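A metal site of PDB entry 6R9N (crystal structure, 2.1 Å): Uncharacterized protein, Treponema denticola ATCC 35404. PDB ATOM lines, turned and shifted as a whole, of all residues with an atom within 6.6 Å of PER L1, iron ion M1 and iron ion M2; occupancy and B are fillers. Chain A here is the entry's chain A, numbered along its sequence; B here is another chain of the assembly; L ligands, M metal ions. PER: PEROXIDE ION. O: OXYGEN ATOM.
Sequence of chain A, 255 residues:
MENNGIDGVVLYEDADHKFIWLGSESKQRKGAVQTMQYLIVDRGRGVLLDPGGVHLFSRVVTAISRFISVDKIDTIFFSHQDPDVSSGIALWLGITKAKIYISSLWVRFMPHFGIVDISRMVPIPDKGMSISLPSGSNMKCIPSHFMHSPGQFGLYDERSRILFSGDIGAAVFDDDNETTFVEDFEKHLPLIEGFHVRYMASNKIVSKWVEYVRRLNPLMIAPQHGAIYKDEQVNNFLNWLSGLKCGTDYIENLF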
ATOM      1  N   THR A  35       8.533  -8.203  -7.856  1.00  0.00           N
ATOM      2  CA  THR A  35       8.418  -8.172  -6.408  1.00  0.00           C
ATOM      3  C   THR A  35       7.272  -7.237  -6.029  1.00  0.00           C
ATOM      4  O   THR A  35       6.922  -6.325  -6.774  1.00  0.00           O
ATOM      5  CB  THR A  35       9.727  -7.719  -5.758  1.00  0.00           C
ATOM      6  OG1 THR A  35      10.055  -6.409  -6.252  1.00  0.00           O
ATOM      7  CG2 THR A  35      10.864  -8.673  -6.108  1.00  0.00           C
ATOM      8  N   ASP A  50       9.432  -5.046   2.915  1.00  0.00           N
ATOM      9  CA  ASP A  50      10.308  -5.633   1.895  1.00  0.00           C
ATOM     10  C   ASP A  50      10.470  -4.707   0.702  1.00  0.00           C
ATOM     11  O   ASP A  50      10.006  -5.011  -0.409  1.00  0.00           O
ATOM     12  CB  ASP A  50       9.780  -6.994   1.453  1.00  0.00           C
ATOM     13  CG  ASP A  50      10.096  -8.086   2.455  1.00  0.00           C
ATOM     14  OD1 ASP A  50      10.462  -7.741   3.611  1.00  0.00           O
ATOM     15  OD2 ASP A  50       9.984  -9.290   2.096  1.00  0.00           O
ATOM     16  N   SER A  79      11.410  -9.398   5.520  1.00  0.00           N
ATOM     17  CA  SER A  79      10.973 -10.748   5.833  1.00  0.00           C
ATOM     18  C   SER A  79      12.173 -11.686   6.010  1.00  0.00           C
ATOM     19  O   SER A  79      12.150 -12.579   6.870  1.00  0.00           O
ATOM     20  CB  SER A  79      10.027 -11.280   4.750  1.00  0.00           C
ATOM     21  OG  SER A  79      10.665 -11.365   3.481  1.00  0.00           O
ATOM     22  N   HIS A  80      13.237 -11.497   5.224  1.00  0.00           N
ATOM     23  CA  HIS A  80      14.454 -12.314   5.364  1.00  0.00           C
ATOM     24  C   HIS A  80      15.590 -11.621   4.613  1.00  0.00           C
ATOM     25  O   HIS A  80      15.502 -10.430   4.302  1.00  0.00           O
ATOM     26  CB  HIS A  80      14.202 -13.764   4.881  1.00  0.00           C
ATOM     27  CG  HIS A  80      13.802 -13.878   3.451  1.00  0.00           C
ATOM     28  ND1 HIS A  80      12.667 -13.268   2.933  1.00  0.00           N
ATOM     29  CD2 HIS A  80      14.359 -14.545   2.413  1.00  0.00           C
ATOM     30  CE1 HIS A  80      12.550 -13.567   1.650  1.00  0.00           C
ATOM     31  NE2 HIS A  80      13.580 -14.333   1.309  1.00  0.00           N
ATOM     32  N   GLN A  81      16.643 -12.367   4.285  1.00  0.00           N
ATOM     33  CA  GLN A  81      17.936 -11.813   3.878  1.00  0.00           C
ATOM     34  C   GLN A  81      18.108 -11.663   2.372  1.00  0.00           C
ATOM     35  O   GLN A  81      19.099 -11.067   1.946  1.00  0.00           O
ATOM     36  CB  GLN A  81      19.076 -12.692   4.416  1.00  0.00           C
ATOM     37  CG  GLN A  81      19.443 -13.909   3.525  1.00  0.00           C
ATOM     38  CD  GLN A  81      18.485 -15.092   3.703  1.00  0.00           C
ATOM     39  OE1 GLN A  81      17.406 -14.952   4.321  1.00  0.00           O
ATOM     40  NE2 GLN A  81      18.869 -16.270   3.155  1.00  0.00           N
ATOM     41  N   ASP A  82      17.175 -12.169   1.566  1.00  0.00           N
ATOM     42  CA  ASP A  82      17.399 -12.291   0.136  1.00  0.00           C
ATOM     43  C   ASP A  82      17.576 -10.926  -0.555  1.00  0.00           C
ATOM     44  O   ASP A  82      17.020  -9.920  -0.109  1.00  0.00           O
ATOM     45  CB  ASP A  82      16.246 -13.037  -0.525  1.00  0.00           C
ATOM     46  CG  ASP A  82      16.353 -14.503  -0.351  1.00  0.00           C
ATOM     47  OD1 ASP A  82      17.316 -14.954   0.316  1.00  0.00           O
ATOM     48  OD2 ASP A  82      15.492 -15.209  -0.893  1.00  0.00           O
ATOM     49  N   ASP A  84      16.223  -9.831  -3.361  1.00  0.00           N
ATOM     50  CA  ASP A  84      14.962  -9.220  -3.768  1.00  0.00           C
ATOM     51  C   ASP A  84      14.209  -8.565  -2.609  1.00  0.00           C
ATOM     52  O   ASP A  84      13.244  -7.831  -2.851  1.00  0.00           O
ATOM     53  CB  ASP A  84      14.082 -10.248  -4.490  1.00  0.00           C
ATOM     54  CG  ASP A  84      13.715 -11.434  -3.609  1.00  0.00           C
ATOM     55  OD1 ASP A  84      14.593 -11.896  -2.855  1.00  0.00           O
ATOM     56  OD2 ASP A  84      12.566 -11.923  -3.654  1.00  0.00           O
ATOM     57  N   VAL A  85      14.611  -8.810  -1.368  1.00  0.00           N
ATOM     58  CA  VAL A  85      14.012  -8.193  -0.184  1.00  0.00           C
ATOM     59  C   VAL A  85      14.763  -6.939   0.238  1.00  0.00           C
ATOM     60  O   VAL A  85      14.153  -5.926   0.586  1.00  0.00           O
ATOM     61  CB  VAL A  85      13.954  -9.194   0.993  1.00  0.00           C
ATOM     62  CG1 VAL A  85      13.536  -8.483   2.295  1.00  0.00           C
ATOM     63  CG2 VAL A  85      13.023 -10.351   0.699  1.00  0.00           C
ATOM     64  N   HIS A 148      11.475 -19.996   2.633  1.00  0.00           N
ATOM     65  CA  HIS A 148      12.619 -20.929   2.618  1.00  0.00           C
ATOM     66  C   HIS A 148      13.711 -20.598   3.632  1.00  0.00           C
ATOM     67  O   HIS A 148      14.458 -21.490   4.066  1.00  0.00           O
ATOM     68  CB  HIS A 148      13.267 -20.917   1.238  1.00  0.00           C
ATOM     69  CG  HIS A 148      13.691 -19.546   0.792  1.00  0.00           C
ATOM     70  ND1 HIS A 148      14.962 -19.058   0.996  1.00  0.00           N
ATOM     71  CD2 HIS A 148      13.003 -18.565   0.178  1.00  0.00           C
ATOM     72  CE1 HIS A 148      15.052 -17.838   0.512  1.00  0.00           C
ATOM     73  NE2 HIS A 148      13.872 -17.505   0.006  1.00  0.00           N
ATOM     74  N   SER A 149      13.828 -19.329   3.998  1.00  0.00           N
ATOM     75  CA  SER A 149      15.027 -18.932   4.733  1.00  0.00           C
ATOM     76  C   SER A 149      14.943 -19.378   6.188  1.00  0.00           C
ATOM     77  O   SER A 149      13.861 -19.348   6.784  1.00  0.00           O
ATOM     78  CB  SER A 149      15.204 -17.402   4.674  1.00  0.00           C
ATOM     79  OG  SER A 149      16.081 -16.932   5.674  1.00  0.00           O
ATOM     80  N   GLN A 152      13.063 -16.173   8.754  1.00  0.00           N
ATOM     81  CA  GLN A 152      12.087 -15.421   7.979  1.00  0.00           C
ATOM     82  C   GLN A 152      10.877 -15.143   8.843  1.00  0.00           C
ATOM     83  O   GLN A 152      10.442 -16.016   9.600  1.00  0.00           O
ATOM     84  CB  GLN A 152      11.627 -16.183   6.702  1.00  0.00           C
ATOM     85  CG  GLN A 152      10.494 -15.445   5.925  1.00  0.00           C
ATOM     86  CD  GLN A 152       9.982 -16.170   4.655  1.00  0.00           C
ATOM     87  OE1 GLN A 152       9.935 -15.581   3.563  1.00  0.00           O
ATOM     88  NE2 GLN A 152       9.548 -17.403   4.810  1.00  0.00           N
ATOM     89  N   GLY A 166       5.836 -12.727   3.012  1.00  0.00           N
ATOM     90  CA  GLY A 166       7.143 -12.962   2.441  1.00  0.00           C
ATOM     91  C   GLY A 166       7.049 -13.827   1.190  1.00  0.00           C
ATOM     92  O   GLY A 166       6.215 -13.594   0.324  1.00  0.00           O
ATOM     93  N   ASP A 167       7.934 -14.819   1.092  1.00  0.00           N
ATOM     94  CA  ASP A 167       7.906 -15.718  -0.067  1.00  0.00           C
ATOM     95  C   ASP A 167       6.736 -16.700  -0.025  1.00  0.00           C
ATOM     96  O   ASP A 167       6.510 -17.413  -1.012  1.00  0.00           O
ATOM     97  CB  ASP A 167       9.207 -16.515  -0.171  1.00  0.00           C
ATOM     98  CG  ASP A 167      10.350 -15.695  -0.717  1.00  0.00           C
ATOM     99  OD1 ASP A 167      10.104 -14.672  -1.385  1.00  0.00           O
ATOM    100  OD2 ASP A 167      11.514 -16.078  -0.455  1.00  0.00           O
ATOM    101  N   ALA A 170       4.072 -16.925  -2.824  1.00  0.00           N
ATOM    102  CA  ALA A 170       4.625 -16.210  -3.965  1.00  0.00           C
ATOM    103  C   ALA A 170       4.281 -16.919  -5.264  1.00  0.00           C
ATOM    104  O   ALA A 170       4.332 -18.146  -5.365  1.00  0.00           O
ATOM    105  CB  ALA A 170       6.145 -16.108  -3.832  1.00  0.00           C
ATOM    106  N   VAL A 172       5.762 -16.910  -9.143  1.00  0.00           N
ATOM    107  CA  VAL A 172       7.035 -16.554  -9.763  1.00  0.00           C
ATOM    108  C   VAL A 172       6.928 -16.356 -11.269  1.00  0.00           C
ATOM    109  O   VAL A 172       7.780 -15.674 -11.853  1.00  0.00           O
ATOM    110  CB  VAL A 172       8.099 -17.619  -9.397  1.00  0.00           C
ATOM    111  CG1 VAL A 172       9.240 -17.681 -10.414  1.00  0.00           C
ATOM    112  CG2 VAL A 172       8.623 -17.361  -7.991  1.00  0.00           C
ATOM    113  N   PHE A 195       7.465 -23.345  -7.366  1.00  0.00           N
ATOM    114  CA  PHE A 195       8.197 -22.579  -6.363  1.00  0.00           C
ATOM    115  C   PHE A 195       8.020 -23.175  -4.962  1.00  0.00           C
ATOM    116  O   PHE A 195       8.996 -23.356  -4.224  1.00  0.00           O
ATOM    117  CB  PHE A 195       7.768 -21.115  -6.391  1.00  0.00           C
ATOM    118  CG  PHE A 195       8.498 -20.251  -5.411  1.00  0.00           C
ATOM    119  CD1 PHE A 195       9.757 -19.743  -5.717  1.00  0.00           C
ATOM    120  CD2 PHE A 195       7.929 -19.927  -4.186  1.00  0.00           C
ATOM    121  CE1 PHE A 195      10.430 -18.926  -4.834  1.00  0.00           C
ATOM    122  CE2 PHE A 195       8.609 -19.143  -3.273  1.00  0.00           C
ATOM    123  CZ  PHE A 195       9.852 -18.635  -3.598  1.00  0.00           C
ATOM    124  N   TYR A 199      11.174 -24.732  -3.025  1.00  0.00           N
ATOM    125  CA  TYR A 199      11.799 -23.796  -2.088  1.00  0.00           C
ATOM    126  C   TYR A 199      11.339 -23.960  -0.640  1.00  0.00           C
ATOM    127  O   TYR A 199      12.096 -23.627   0.276  1.00  0.00           O
ATOM    128  CB  TYR A 199      11.551 -22.341  -2.506  1.00  0.00           C
ATOM    129  CG  TYR A 199      12.212 -21.863  -3.788  1.00  0.00           C
ATOM    130  CD1 TYR A 199      11.833 -22.367  -5.030  1.00  0.00           C
ATOM    131  CD2 TYR A 199      13.174 -20.858  -3.752  1.00  0.00           C
ATOM    132  CE1 TYR A 199      12.424 -21.901  -6.205  1.00  0.00           C
ATOM    133  CE2 TYR A 199      13.775 -20.386  -4.915  1.00  0.00           C
ATOM    134  CZ  TYR A 199      13.391 -20.913  -6.137  1.00  0.00           C
ATOM    135  OH  TYR A 199      13.978 -20.427  -7.288  1.00  0.00           O
ATOM    136  N   GLN A 224       5.262 -11.581  -1.207  1.00  0.00           N
ATOM    137  CA  GLN A 224       6.305 -10.748  -1.755  1.00  0.00           C
ATOM    138  C   GLN A 224       6.398 -10.857  -3.282  1.00  0.00           C
ATOM    139  O   GLN A 224       7.100 -10.057  -3.902  1.00  0.00           O
ATOM    140  CB  GLN A 224       7.645 -11.118  -1.081  1.00  0.00           C
ATOM    141  CG  GLN A 224       8.728 -10.081  -1.150  1.00  0.00           C
ATOM    142  CD  GLN A 224       9.994 -10.641  -1.767  1.00  0.00           C
ATOM    143  OE1 GLN A 224      10.372 -11.795  -1.490  1.00  0.00           O
ATOM    144  NE2 GLN A 224      10.648  -9.846  -2.618  1.00  0.00           N
ATOM    145  N   HIS A 225       5.710 -11.831  -3.887  1.00  0.00           N
ATOM    146  CA  HIS A 225       5.618 -11.967  -5.340  1.00  0.00           C
ATOM    147  C   HIS A 225       4.215 -12.403  -5.731  1.00  0.00           C
ATOM    148  O   HIS A 225       3.694 -13.368  -5.182  1.00  0.00           O
ATOM    149  CB  HIS A 225       6.616 -13.003  -5.902  1.00  0.00           C
ATOM    150  CG  HIS A 225       7.996 -12.915  -5.338  1.00  0.00           C
ATOM    151  ND1 HIS A 225       8.974 -12.101  -5.869  1.00  0.00           N
ATOM    152  CD2 HIS A 225       8.581 -13.569  -4.303  1.00  0.00           C
ATOM    153  CE1 HIS A 225      10.085 -12.234  -5.178  1.00  0.00           C
ATOM    154  NE2 HIS A 225       9.870 -13.117  -4.217  1.00  0.00           N
ATOM    155  N   GLN B  81      22.561 -17.342  -2.538  1.00  0.00           N
ATOM    156  CA  GLN B  81      22.053 -16.024  -2.899  1.00  0.00           C
ATOM    157  C   GLN B  81      22.383 -14.936  -1.886  1.00  0.00           C
ATOM    158  O   GLN B  81      22.198 -13.763  -2.195  1.00  0.00           O
ATOM    159  CB  GLN B  81      20.526 -16.093  -3.062  1.00  0.00           C
ATOM    160  CG  GLN B  81      19.750 -16.024  -1.726  1.00  0.00           C
ATOM    161  CD  GLN B  81      19.736 -17.349  -0.973  1.00  0.00           C
ATOM    162  OE1 GLN B  81      20.476 -18.306  -1.279  1.00  0.00           O
ATOM    163  NE2 GLN B  81      18.849 -17.423   0.015  1.00  0.00           N
ATOM    164  N   LEU B 105      17.954 -21.813  -9.020  1.00  0.00           N
ATOM    165  CA  LEU B 105      16.926 -21.225  -8.160  1.00  0.00           C
ATOM    166  C   LEU B 105      17.063 -19.719  -8.047  1.00  0.00           C
ATOM    167  O   LEU B 105      16.076 -19.026  -7.761  1.00  0.00           O
ATOM    168  CB  LEU B 105      16.969 -21.853  -6.768  1.00  0.00           C
ATOM    169  CG  LEU B 105      16.082 -23.059  -6.490  1.00  0.00           C
ATOM    170  CD1 LEU B 105      16.582 -24.276  -7.253  1.00  0.00           C
ATOM    171  CD2 LEU B 105      16.054 -23.378  -4.998  1.00  0.00           C
ATOM    172  N   TRP B 106      18.269 -19.183  -8.224  1.00  0.00           N
ATOM    173  CA  TRP B 106      18.570 -17.802  -7.912  1.00  0.00           C
ATOM    174  C   TRP B 106      18.842 -16.914  -9.123  1.00  0.00           C
ATOM    175  O   TRP B 106      18.945 -15.695  -8.964  1.00  0.00           O
ATOM    176  CB  TRP B 106      19.772 -17.734  -6.956  1.00  0.00           C
ATOM    177  CG  TRP B 106      19.559 -18.525  -5.728  1.00  0.00           C
ATOM    178  CD1 TRP B 106      20.350 -19.514  -5.243  1.00  0.00           C
ATOM    179  CD2 TRP B 106      18.464 -18.414  -4.821  1.00  0.00           C
ATOM    180  NE1 TRP B 106      19.825 -20.032  -4.086  1.00  0.00           N
ATOM    181  CE2 TRP B 106      18.653 -19.368  -3.806  1.00  0.00           C
ATOM    182  CE3 TRP B 106      17.337 -17.592  -4.760  1.00  0.00           C
ATOM    183  CZ2 TRP B 106      17.763 -19.533  -2.743  1.00  0.00           C
ATOM    184  CZ3 TRP B 106      16.437 -17.765  -3.732  1.00  0.00           C
ATOM    185  CH2 TRP B 106      16.655 -18.719  -2.730  1.00  0.00           C
ATOM    186  N   PHE B 109      16.687 -13.895  -9.530  1.00  0.00           N
ATOM    187  CA  PHE B 109      16.460 -13.110  -8.333  1.00  0.00           C
ATOM    188  C   PHE B 109      17.658 -12.223  -7.966  1.00  0.00           C
ATOM    189  O   PHE B 109      17.660 -11.650  -6.870  1.00  0.00           O
ATOM    190  CB  PHE B 109      16.139 -14.020  -7.146  1.00  0.00           C
ATOM    191  CG  PHE B 109      14.826 -14.772  -7.270  1.00  0.00           C
ATOM    192  CD1 PHE B 109      13.642 -14.202  -6.871  1.00  0.00           C
ATOM    193  CD2 PHE B 109      14.807 -16.084  -7.740  1.00  0.00           C
ATOM    194  CE1 PHE B 109      12.437 -14.904  -6.972  1.00  0.00           C
ATOM    195  CE2 PHE B 109      13.628 -16.783  -7.831  1.00  0.00           C
ATOM    196  CZ  PHE B 109      12.438 -16.195  -7.443  1.00  0.00           C
HETATM  197  O1  PER L   1      12.163 -15.466  -3.574  1.00  0.00           O
HETATM  198  O2  PER L   1      13.204 -16.300  -2.910  1.00  0.00           O
HETATM  199  O     O L   2      13.093 -13.549  -1.431  1.00  0.00           O
HETATM  200 FE    FE M   1      11.431 -13.487  -2.669  1.00  0.00          FE
HETATM  201 FE    FE M   2      13.494 -15.493  -0.782  1.00  0.00          FE
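OD1 of Asp 82 is in hydrogen-bond range of NE2 of Gln 81 of chain B, 2.9 Å away.
OD1 of Asp 82 is in hydrogen-bond range of NE2 of Gln 81 of chain A, at 3.5 Å.
OE1 of Gln 152 lies within hydrogen-bond range of N of Asp 167 (3.3 Å).
N of Gln 224 is in hydrogen-bond range of O of Gly 166 (2.7 Å).
A ring nitrogen (ND1) of His 80 is in hydrogen-bond range of the side-chain hydroxyl of Ser 79.
The indole nitrogen of Trp 106 of chain B sits close to the side-chain amide oxygen of Gln 81 of chain B, 3.4 Å away.
Merely in contact with PER L1: Phe 109 of chain B (3.5 Å), Trp 106 of chain B (3.6 Å) and Phe 195 (3.9 Å).
Hydrophobic or aromatic side chains within 4 Å of PER L1: His 148, Phe 195, Trp 106 of chain B and Phe 109 of chain B.
Within 4 Å of iron ion M1: Asp 84, Asp 167, Gln 224 and His 225.
Of the 23 residues printed, 4 come within 4 Å of iron ion M2.
Along chain A the residues within 4 Å of iron ion M2 span positions 80 to 167.
The nearest printed residue that does not touch iron ion M2 is Asp 84 (4.3 Å).
Iron ion M1 is bound by an oxygen (O) of O L2 (2.1 Å), the side-chain carboxylate (OD2) of Asp 84 (2.2 Å), the side-chain carboxylate (OD1) of Asp 167 (2.2 Å), a ring nitrogen (NE2) of His 225 (2.2 Å), an oxygen (O1) of PER L1 (2.3 Å) and the side-chain amide oxygen (OE1) of Gln 224 (2.3 Å).
Iron ion M1 has six donor atoms within binding distance.
Iron ion M2 is bound by the side-chain carboxylate (OD2) of Asp 82 (2.0 Å), an oxygen (O) of O L2 (2.1 Å), the side-chain carboxylate (OD2) of Asp 167 (2.1 Å), a ring nitrogen (NE2) of His 148 (2.2 Å), an oxygen (O2) of PER L1 (2.3 Å) and a ring nitrogen (NE2) of His 80 (2.4 Å).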
